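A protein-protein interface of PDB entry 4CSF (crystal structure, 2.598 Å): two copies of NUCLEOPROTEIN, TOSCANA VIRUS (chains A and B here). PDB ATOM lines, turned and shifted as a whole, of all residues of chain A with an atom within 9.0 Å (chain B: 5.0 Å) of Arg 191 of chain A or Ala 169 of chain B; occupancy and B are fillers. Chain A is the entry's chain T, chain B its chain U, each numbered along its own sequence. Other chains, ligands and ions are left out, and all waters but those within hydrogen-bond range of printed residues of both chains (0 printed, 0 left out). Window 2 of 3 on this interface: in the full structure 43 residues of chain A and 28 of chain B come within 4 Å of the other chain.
O of Lys 184 of chain A touches CE of Met 207 of chain B (3.7 Å). Thr 185 of chain A touches Met 207 of chain B (CA to CE, 3.9 Å). Met 207 of chain B touches Pro 188 of chain A. Ala 172 of chain B touches Arg 191 of chain A. Asp 173 of chain B touches Thr 192 of chain A. Tyr 247 of chain B touches Thr 192 of chain A (CE2 to CG2, 3.7 Å).
Hydrophobic or aromatic side chains of chain B within 4 Å of the printed part of chain A: Ala 169, Ala 172, Met 207 and Tyr 247. Hydrophobic or aromatic side chains of chain A within 4 Å of the printed part of chain B: Pro 188. Among the printed residues, Asp or Glu carboxylates within 4 Å of a Lys or Arg side-chain nitrogen of the other chain: Arg 191 of chain A with Asp 173 of chain B.
NH2 of Arg 191 of chain A is in salt-bridge range of OD1 of Asp 173 of chain B, at 2.6 Å. O of Ala 169 of chain B is in hydrogen-bond range of NH1 of Arg 191 of chain A.
No position is printed for both chains.
Arg 191 of chain A touches three residues of chain B. Ala 169 of chain B touches one residue of chain A. No residue of chain A comes within 4 Å of Thr 170 of chain B. Printed residues of chain A within 4 Å of Asp 173 of chain B: Arg 191 (2.6 Å) and Thr 192 (3.3 Å). Of the printed residues of chain A, Tyr 247 of chain B touches Thr 192. The nearest residue of chain B that does not touch Arg 191 of chain A is Met 207 of chain B (4.2 Å). The nearest printed residue of chain B that does not touch Lys 184 of chain A is Ala 169 of chain B (6.4 Å).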
ATOM      1  N   ILE A 180      10.927  -8.915  21.219  1.00  0.00           N
ATOM      2  CA  ILE A 180      11.239  -9.872  20.159  1.00  0.00           C
ATOM      3  C   ILE A 180      12.518  -9.465  19.441  1.00  0.00           C
ATOM      4  O   ILE A 180      13.327 -10.314  19.074  1.00  0.00           O
ATOM      5  CB  ILE A 180      10.075 -10.066  19.150  1.00  0.00           C
ATOM      6  CG1 ILE A 180       9.677  -8.741  18.507  1.00  0.00           C
ATOM      7  CG2 ILE A 180       8.869 -10.700  19.829  1.00  0.00           C
ATOM      8  CD1 ILE A 180       8.403  -8.826  17.691  1.00  0.00           C
ATOM      9  N   GLU A 181      12.705  -8.160  19.264  1.00  0.00           N
ATOM     10  CA  GLU A 181      13.897  -7.639  18.604  1.00  0.00           C
ATOM     11  C   GLU A 181      15.121  -7.771  19.496  1.00  0.00           C
ATOM     12  O   GLU A 181      16.191  -8.159  19.042  1.00  0.00           O
ATOM     13  CB  GLU A 181      13.680  -6.184  18.188  1.00  0.00           C
ATOM     14  CG  GLU A 181      12.529  -6.029  17.215  1.00  0.00           C
ATOM     15  CD  GLU A 181      12.721  -6.861  15.954  1.00  0.00           C
ATOM     16  OE1 GLU A 181      13.848  -6.870  15.407  1.00  0.00           O
ATOM     17  OE2 GLU A 181      11.744  -7.502  15.511  1.00  0.00           O
ATOM     18  N   SER A 183      15.491  -9.966  21.892  1.00  0.00           N
ATOM     19  CA  SER A 183      15.803 -11.390  21.975  1.00  0.00           C
ATOM     20  C   SER A 183      16.542 -11.872  20.733  1.00  0.00           C
ATOM     21  O   SER A 183      17.405 -12.745  20.824  1.00  0.00           O
ATOM     22  CB  SER A 183      14.531 -12.216  22.167  1.00  0.00           C
ATOM     23  OG  SER A 183      13.875 -11.871  23.381  1.00  0.00           O
ATOM     24  N   LYS A 184      16.204 -11.292  19.580  1.00  0.00           N
ATOM     25  CA  LYS A 184      16.804 -11.681  18.306  1.00  0.00           C
ATOM     26  C   LYS A 184      18.269 -11.272  18.182  1.00  0.00           C
ATOM     27  O   LYS A 184      19.021 -11.906  17.440  1.00  0.00           O
ATOM     28  CB  LYS A 184      16.018 -11.086  17.136  1.00  0.00           C
ATOM     29  CG  LYS A 184      14.857 -11.928  16.628  1.00  0.00           C
ATOM     30  CD  LYS A 184      14.110 -11.181  15.521  1.00  0.00           C
ATOM     31  CE  LYS A 184      13.080 -12.069  14.841  1.00  0.00           C
ATOM     32  NZ  LYS A 184      12.363 -11.347  13.750  1.00  0.00           N
ATOM     33  N   THR A 185      18.674 -10.206  18.875  1.00  0.00           N
ATOM     34  CA  THR A 185      20.059  -9.748  18.756  1.00  0.00           C
ATOM     35  C   THR A 185      20.959 -10.354  19.833  1.00  0.00           C
ATOM     36  O   THR A 185      22.069 -10.787  19.533  1.00  0.00           O
ATOM     37  CB  THR A 185      20.213  -8.195  18.695  1.00  0.00           C
ATOM     38  OG1 THR A 185      20.302  -7.659  20.018  1.00  0.00           O
ATOM     39  CG2 THR A 185      19.056  -7.552  17.944  1.00  0.00           C
ATOM     40  N   ILE A 186      20.483 -10.414  21.074  1.00  0.00           N
ATOM     41  CA  ILE A 186      21.287 -11.031  22.134  1.00  0.00           C
ATOM     42  C   ILE A 186      21.368 -12.552  21.975  1.00  0.00           C
ATOM     43  O   ILE A 186      22.308 -13.187  22.452  1.00  0.00           O
ATOM     44  CB  ILE A 186      20.810 -10.662  23.559  1.00  0.00           C
ATOM     45  CG1 ILE A 186      19.505 -11.376  23.893  1.00  0.00           C
ATOM     46  CG2 ILE A 186      20.701  -9.144  23.716  1.00  0.00           C
ATOM     47  CD1 ILE A 186      19.101 -11.260  25.349  1.00  0.00           C
ATOM     48  N   ASN A 187      20.376 -13.124  21.299  1.00  0.00           N
ATOM     49  CA  ASN A 187      20.397 -14.539  20.943  1.00  0.00           C
ATOM     50  C   ASN A 187      20.082 -14.745  19.455  1.00  0.00           C
ATOM     51  O   ASN A 187      18.962 -15.124  19.092  1.00  0.00           O
ATOM     52  CB  ASN A 187      19.429 -15.331  21.825  1.00  0.00           C
ATOM     53  CG  ASN A 187      19.626 -16.834  21.709  1.00  0.00           C
ATOM     54  OD1 ASN A 187      20.638 -17.307  21.185  1.00  0.00           O
ATOM     55  ND2 ASN A 187      18.656 -17.594  22.205  1.00  0.00           N
ATOM     56  N   PRO A 188      21.089 -14.507  18.594  1.00  0.00           N
ATOM     57  CA  PRO A 188      20.993 -14.464  17.127  1.00  0.00           C
ATOM     58  C   PRO A 188      20.463 -15.750  16.504  1.00  0.00           C
ATOM     59  O   PRO A 188      20.113 -15.754  15.321  1.00  0.00           O
ATOM     60  CB  PRO A 188      22.443 -14.250  16.690  1.00  0.00           C
ATOM     61  CG  PRO A 188      23.129 -13.657  17.886  1.00  0.00           C
ATOM     62  CD  PRO A 188      22.469 -14.278  19.062  1.00  0.00           C
ATOM     63  N   SER A 189      20.418 -16.829  17.277  1.00  0.00           N
ATOM     64  CA  SER A 189      19.888 -18.093  16.772  1.00  0.00           C
ATOM     65  C   SER A 189      18.382 -17.996  16.548  1.00  0.00           C
ATOM     66  O   SER A 189      17.807 -18.762  15.769  1.00  0.00           O
ATOM     67  CB  SER A 189      20.216 -19.243  17.732  1.00  0.00           C
ATOM     68  OG  SER A 189      19.658 -19.016  19.017  1.00  0.00           O
ATOM     69  N   LEU A 190      17.756 -17.038  17.227  1.00  0.00           N
ATOM     70  CA  LEU A 190      16.314 -16.816  17.127  1.00  0.00           C
ATOM     71  C   LEU A 190      15.912 -15.970  15.913  1.00  0.00           C
ATOM     72  O   LEU A 190      14.725 -15.815  15.630  1.00  0.00           O
ATOM     73  CB  LEU A 190      15.797 -16.151  18.407  1.00  0.00           C
ATOM     74  CG  LEU A 190      16.080 -16.890  19.719  1.00  0.00           C
ATOM     75  CD1 LEU A 190      15.614 -16.083  20.928  1.00  0.00           C
ATOM     76  CD2 LEU A 190      15.427 -18.265  19.707  1.00  0.00           C
ATOM     77  N   ARG A 191      16.901 -15.430  15.202  1.00  0.00           N
ATOM     78  CA  ARG A 191      16.644 -14.488  14.106  1.00  0.00           C
ATOM     79  C   ARG A 191      15.829 -15.116  12.974  1.00  0.00           C
ATOM     80  O   ARG A 191      15.042 -14.439  12.307  1.00  0.00           O
ATOM     81  CB  ARG A 191      17.960 -13.917  13.565  1.00  0.00           C
ATOM     82  CG  ARG A 191      17.795 -12.709  12.661  1.00  0.00           C
ATOM     83  CD  ARG A 191      19.095 -12.374  11.960  1.00  0.00           C
ATOM     84  NE  ARG A 191      19.543 -13.478  11.120  1.00  0.00           N
ATOM     85  CZ  ARG A 191      19.082 -13.717   9.898  1.00  0.00           C
ATOM     86  NH1 ARG A 191      18.159 -12.925   9.368  1.00  0.00           N
ATOM     87  NH2 ARG A 191      19.548 -14.743   9.198  1.00  0.00           N
ATOM     88  N   THR A 192      16.008 -16.418  12.786  1.00  0.00           N
ATOM     89  CA  THR A 192      15.343 -17.142  11.712  1.00  0.00           C
ATOM     90  C   THR A 192      14.024 -17.777  12.161  1.00  0.00           C
ATOM     91  O   THR A 192      13.314 -18.386  11.356  1.00  0.00           O
ATOM     92  CB  THR A 192      16.253 -18.238  11.142  1.00  0.00           C
ATOM     93  OG1 THR A 192      16.771 -19.031  12.217  1.00  0.00           O
ATOM     94  CG2 THR A 192      17.413 -17.621  10.373  1.00  0.00           C
ATOM     95  N   LYS A 193      13.702 -17.631  13.446  1.00  0.00           N
ATOM     96  CA  LYS A 193      12.453 -18.158  13.996  1.00  0.00           C
ATOM     97  C   LYS A 193      11.276 -17.222  13.723  1.00  0.00           C
ATOM     98  O   LYS A 193      11.460 -16.031  13.472  1.00  0.00           O
ATOM     99  CB  LYS A 193      12.579 -18.381  15.504  1.00  0.00           C
ATOM    100  CG  LYS A 193      13.691 -19.335  15.936  1.00  0.00           C
ATOM    101  CD  LYS A 193      13.339 -20.781  15.619  1.00  0.00           C
ATOM    102  CE  LYS A 193      14.392 -21.743  16.158  1.00  0.00           C
ATOM    103  NZ  LYS A 193      14.045 -23.174  15.896  1.00  0.00           N
ATOM    104  N   GLN A 194      10.064 -17.767  13.774  1.00  0.00           N
ATOM    105  CA  GLN A 194       8.861 -16.959  13.625  1.00  0.00           C
ATOM    106  C   GLN A 194       8.684 -16.067  14.852  1.00  0.00           C
ATOM    107  O   GLN A 194       9.168 -16.394  15.938  1.00  0.00           O
ATOM    108  CB  GLN A 194       7.634 -17.850  13.428  1.00  0.00           C
ATOM    109  CG  GLN A 194       7.680 -18.727  12.180  1.00  0.00           C
ATOM    110  CD  GLN A 194       7.693 -17.916  10.897  1.00  0.00           C
ATOM    111  OE1 GLN A 194       6.947 -16.944  10.756  1.00  0.00           O
ATOM    112  NE2 GLN A 194       8.546 -18.308   9.954  1.00  0.00           N
ATOM    113  N   ALA A 195       7.997 -14.942  14.672  1.00  0.00           N
ATOM    114  CA  ALA A 195       7.804 -13.970  15.744  1.00  0.00           C
ATOM    115  C   ALA A 195       7.140 -14.589  16.970  1.00  0.00           C
ATOM    116  O   ALA A 195       7.526 -14.307  18.104  1.00  0.00           O
ATOM    117  CB  ALA A 195       6.997 -12.786  15.240  1.00  0.00           C
ATOM    118  N   GLU A 197       7.272 -17.708  17.890  1.00  0.00           N
ATOM    119  CA  GLU A 197       8.236 -18.618  18.502  1.00  0.00           C
ATOM    120  C   GLU A 197       9.213 -17.835  19.377  1.00  0.00           C
ATOM    121  O   GLU A 197       9.574 -18.278  20.465  1.00  0.00           O
ATOM    122  CB  GLU A 197       8.993 -19.412  17.433  1.00  0.00           C
ATOM    123  CG  GLU A 197       8.111 -20.296  16.562  1.00  0.00           C
ATOM    124  CD  GLU A 197       8.888 -21.004  15.459  1.00  0.00           C
ATOM    125  OE1 GLU A 197       9.656 -20.330  14.736  1.00  0.00           O
ATOM    126  OE2 GLU A 197       8.726 -22.237  15.317  1.00  0.00           O
ATOM    127  N   VAL A 198       9.634 -16.668  18.895  1.00  0.00           N
ATOM    128  CA  VAL A 198      10.555 -15.818  19.641  1.00  0.00           C
ATOM    129  C   VAL A 198       9.873 -15.305  20.906  1.00  0.00           C
ATOM    130  O   VAL A 198      10.472 -15.288  21.986  1.00  0.00           O
ATOM    131  CB  VAL A 198      11.035 -14.626  18.797  1.00  0.00           C
ATOM    132  CG1 VAL A 198      11.926 -13.703  19.626  1.00  0.00           C
ATOM    133  CG2 VAL A 198      11.764 -15.114  17.542  1.00  0.00           C
ATOM    134  N   LEU B 161      20.015  -4.777   8.840  1.00  0.00           N
ATOM    135  CA  LEU B 161      18.936  -5.655   9.286  1.00  0.00           C
ATOM    136  C   LEU B 161      17.598  -4.924   9.375  1.00  0.00           C
ATOM    137  O   LEU B 161      16.545  -5.555   9.460  1.00  0.00           O
ATOM    138  CB  LEU B 161      19.284  -6.283  10.638  1.00  0.00           C
ATOM    139  CG  LEU B 161      20.406  -7.321  10.633  1.00  0.00           C
ATOM    140  CD1 LEU B 161      20.944  -7.536  12.038  1.00  0.00           C
ATOM    141  CD2 LEU B 161      19.921  -8.640  10.036  1.00  0.00           C
ATOM    142  N   GLY B 166      11.518  -6.708   5.972  1.00  0.00           N
ATOM    143  CA  GLY B 166      12.360  -7.830   6.342  1.00  0.00           C
ATOM    144  C   GLY B 166      13.401  -8.173   5.295  1.00  0.00           C
ATOM    145  O   GLY B 166      13.899  -9.300   5.250  1.00  0.00           O
ATOM    146  N   ALA B 167      13.732  -7.205   4.445  1.00  0.00           N
ATOM    147  CA  ALA B 167      14.739  -7.418   3.414  1.00  0.00           C
ATOM    148  C   ALA B 167      16.094  -7.732   4.046  1.00  0.00           C
ATOM    149  O   ALA B 167      16.827  -8.605   3.570  1.00  0.00           O
ATOM    150  CB  ALA B 167      14.836  -6.206   2.507  1.00  0.00           C
ATOM    151  N   GLY B 168      16.416  -7.021   5.125  1.00  0.00           N
ATOM    152  CA  GLY B 168      17.662  -7.238   5.843  1.00  0.00           C
ATOM    153  C   GLY B 168      17.767  -8.651   6.393  1.00  0.00           C
ATOM    154  O   GLY B 168      18.835  -9.273   6.337  1.00  0.00           O
ATOM    155  N   ALA B 169      16.656  -9.162   6.918  1.00  0.00           N
ATOM    156  CA  ALA B 169      16.625 -10.517   7.458  1.00  0.00           C
ATOM    157  C   ALA B 169      16.854 -11.529   6.344  1.00  0.00           C
ATOM    158  O   ALA B 169      17.567 -12.520   6.523  1.00  0.00           O
ATOM    159  CB  ALA B 169      15.303 -10.777   8.148  1.00  0.00           C
ATOM    160  N   THR B 170      16.252 -11.262   5.191  1.00  0.00           N
ATOM    161  CA  THR B 170      16.383 -12.143   4.041  1.00  0.00           C
ATOM    162  C   THR B 170      17.830 -12.163   3.542  1.00  0.00           C
ATOM    163  O   THR B 170      18.381 -13.230   3.248  1.00  0.00           O
ATOM    164  CB  THR B 170      15.427 -11.719   2.918  1.00  0.00           C
ATOM    165  OG1 THR B 170      14.086 -11.701   3.422  1.00  0.00           O
ATOM    166  CG2 THR B 170      15.508 -12.679   1.746  1.00  0.00           C
ATOM    167  N   ILE B 171      18.444 -10.982   3.465  1.00  0.00           N
ATOM    168  CA  ILE B 171      19.852 -10.872   3.084  1.00  0.00           C
ATOM    169  C   ILE B 171      20.739 -11.665   4.056  1.00  0.00           C
ATOM    170  O   ILE B 171      21.660 -12.379   3.635  1.00  0.00           O
ATOM    171  CB  ILE B 171      20.316  -9.400   3.008  1.00  0.00           C
ATOM    172  CG1 ILE B 171      19.564  -8.655   1.901  1.00  0.00           C
ATOM    173  CG2 ILE B 171      21.818  -9.317   2.764  1.00  0.00           C
ATOM    174  CD1 ILE B 171      19.817  -7.155   1.861  1.00  0.00           C
ATOM    175  N   ALA B 172      20.453 -11.543   5.349  1.00  0.00           N
ATOM    176  CA  ALA B 172      21.195 -12.279   6.371  1.00  0.00           C
ATOM    177  C   ALA B 172      21.011 -13.794   6.221  1.00  0.00           C
ATOM    178  O   ALA B 172      21.958 -14.558   6.394  1.00  0.00           O
ATOM    179  CB  ALA B 172      20.779 -11.827   7.744  1.00  0.00           C
ATOM    180  N   ASP B 173      19.795 -14.221   5.890  1.00  0.00           N
ATOM    181  CA  ASP B 173      19.532 -15.635   5.627  1.00  0.00           C
ATOM    182  C   ASP B 173      20.370 -16.135   4.454  1.00  0.00           C
ATOM    183  O   ASP B 173      21.009 -17.187   4.546  1.00  0.00           O
ATOM    184  CB  ASP B 173      18.045 -15.876   5.342  1.00  0.00           C
ATOM    185  CG  ASP B 173      17.170 -15.656   6.561  1.00  0.00           C
ATOM    186  OD1 ASP B 173      17.702 -15.701   7.694  1.00  0.00           O
ATOM    187  OD2 ASP B 173      15.946 -15.447   6.390  1.00  0.00           O
ATOM    188  N   MET B 207      26.274 -11.706  14.193  1.00  0.00           N
ATOM    189  CA  MET B 207      25.308 -10.699  14.629  1.00  0.00           C
ATOM    190  C   MET B 207      26.009  -9.411  15.046  1.00  0.00           C
ATOM    191  O   MET B 207      25.512  -8.312  14.781  1.00  0.00           O
ATOM    192  CB  MET B 207      24.463 -11.210  15.793  1.00  0.00           C
ATOM    193  CG  MET B 207      22.960 -11.116  15.568  1.00  0.00           C
ATOM    194  SD  MET B 207      22.374  -9.483  15.131  1.00  0.00           S
ATOM    195  CE  MET B 207      20.632  -9.808  14.900  1.00  0.00           C
ATOM    196  N   TYR B 247      18.425 -21.631   3.118  1.00  0.00           N
ATOM    197  CA  TYR B 247      19.029 -21.525   4.439  1.00  0.00           C
ATOM    198  C   TYR B 247      18.020 -21.791   5.541  1.00  0.00           C
ATOM    199  O   TYR B 247      18.301 -22.546   6.473  1.00  0.00           O
ATOM    200  CB  TYR B 247      19.642 -20.140   4.620  1.00  0.00           C
ATOM    201  CG  TYR B 247      20.214 -19.899   5.994  1.00  0.00           C
ATOM    202  CD1 TYR B 247      21.407 -20.496   6.386  1.00  0.00           C
ATOM    203  CD2 TYR B 247      19.573 -19.063   6.900  1.00  0.00           C
ATOM    204  CE1 TYR B 247      21.945 -20.273   7.649  1.00  0.00           C
ATOM    205  CE2 TYR B 247      20.104 -18.834   8.164  1.00  0.00           C
ATOM    206  CZ  TYR B 247      21.290 -19.440   8.530  1.00  0.00           C
ATOM    207  OH  TYR B 247      21.818 -19.210   9.784  1.00  0.00           O
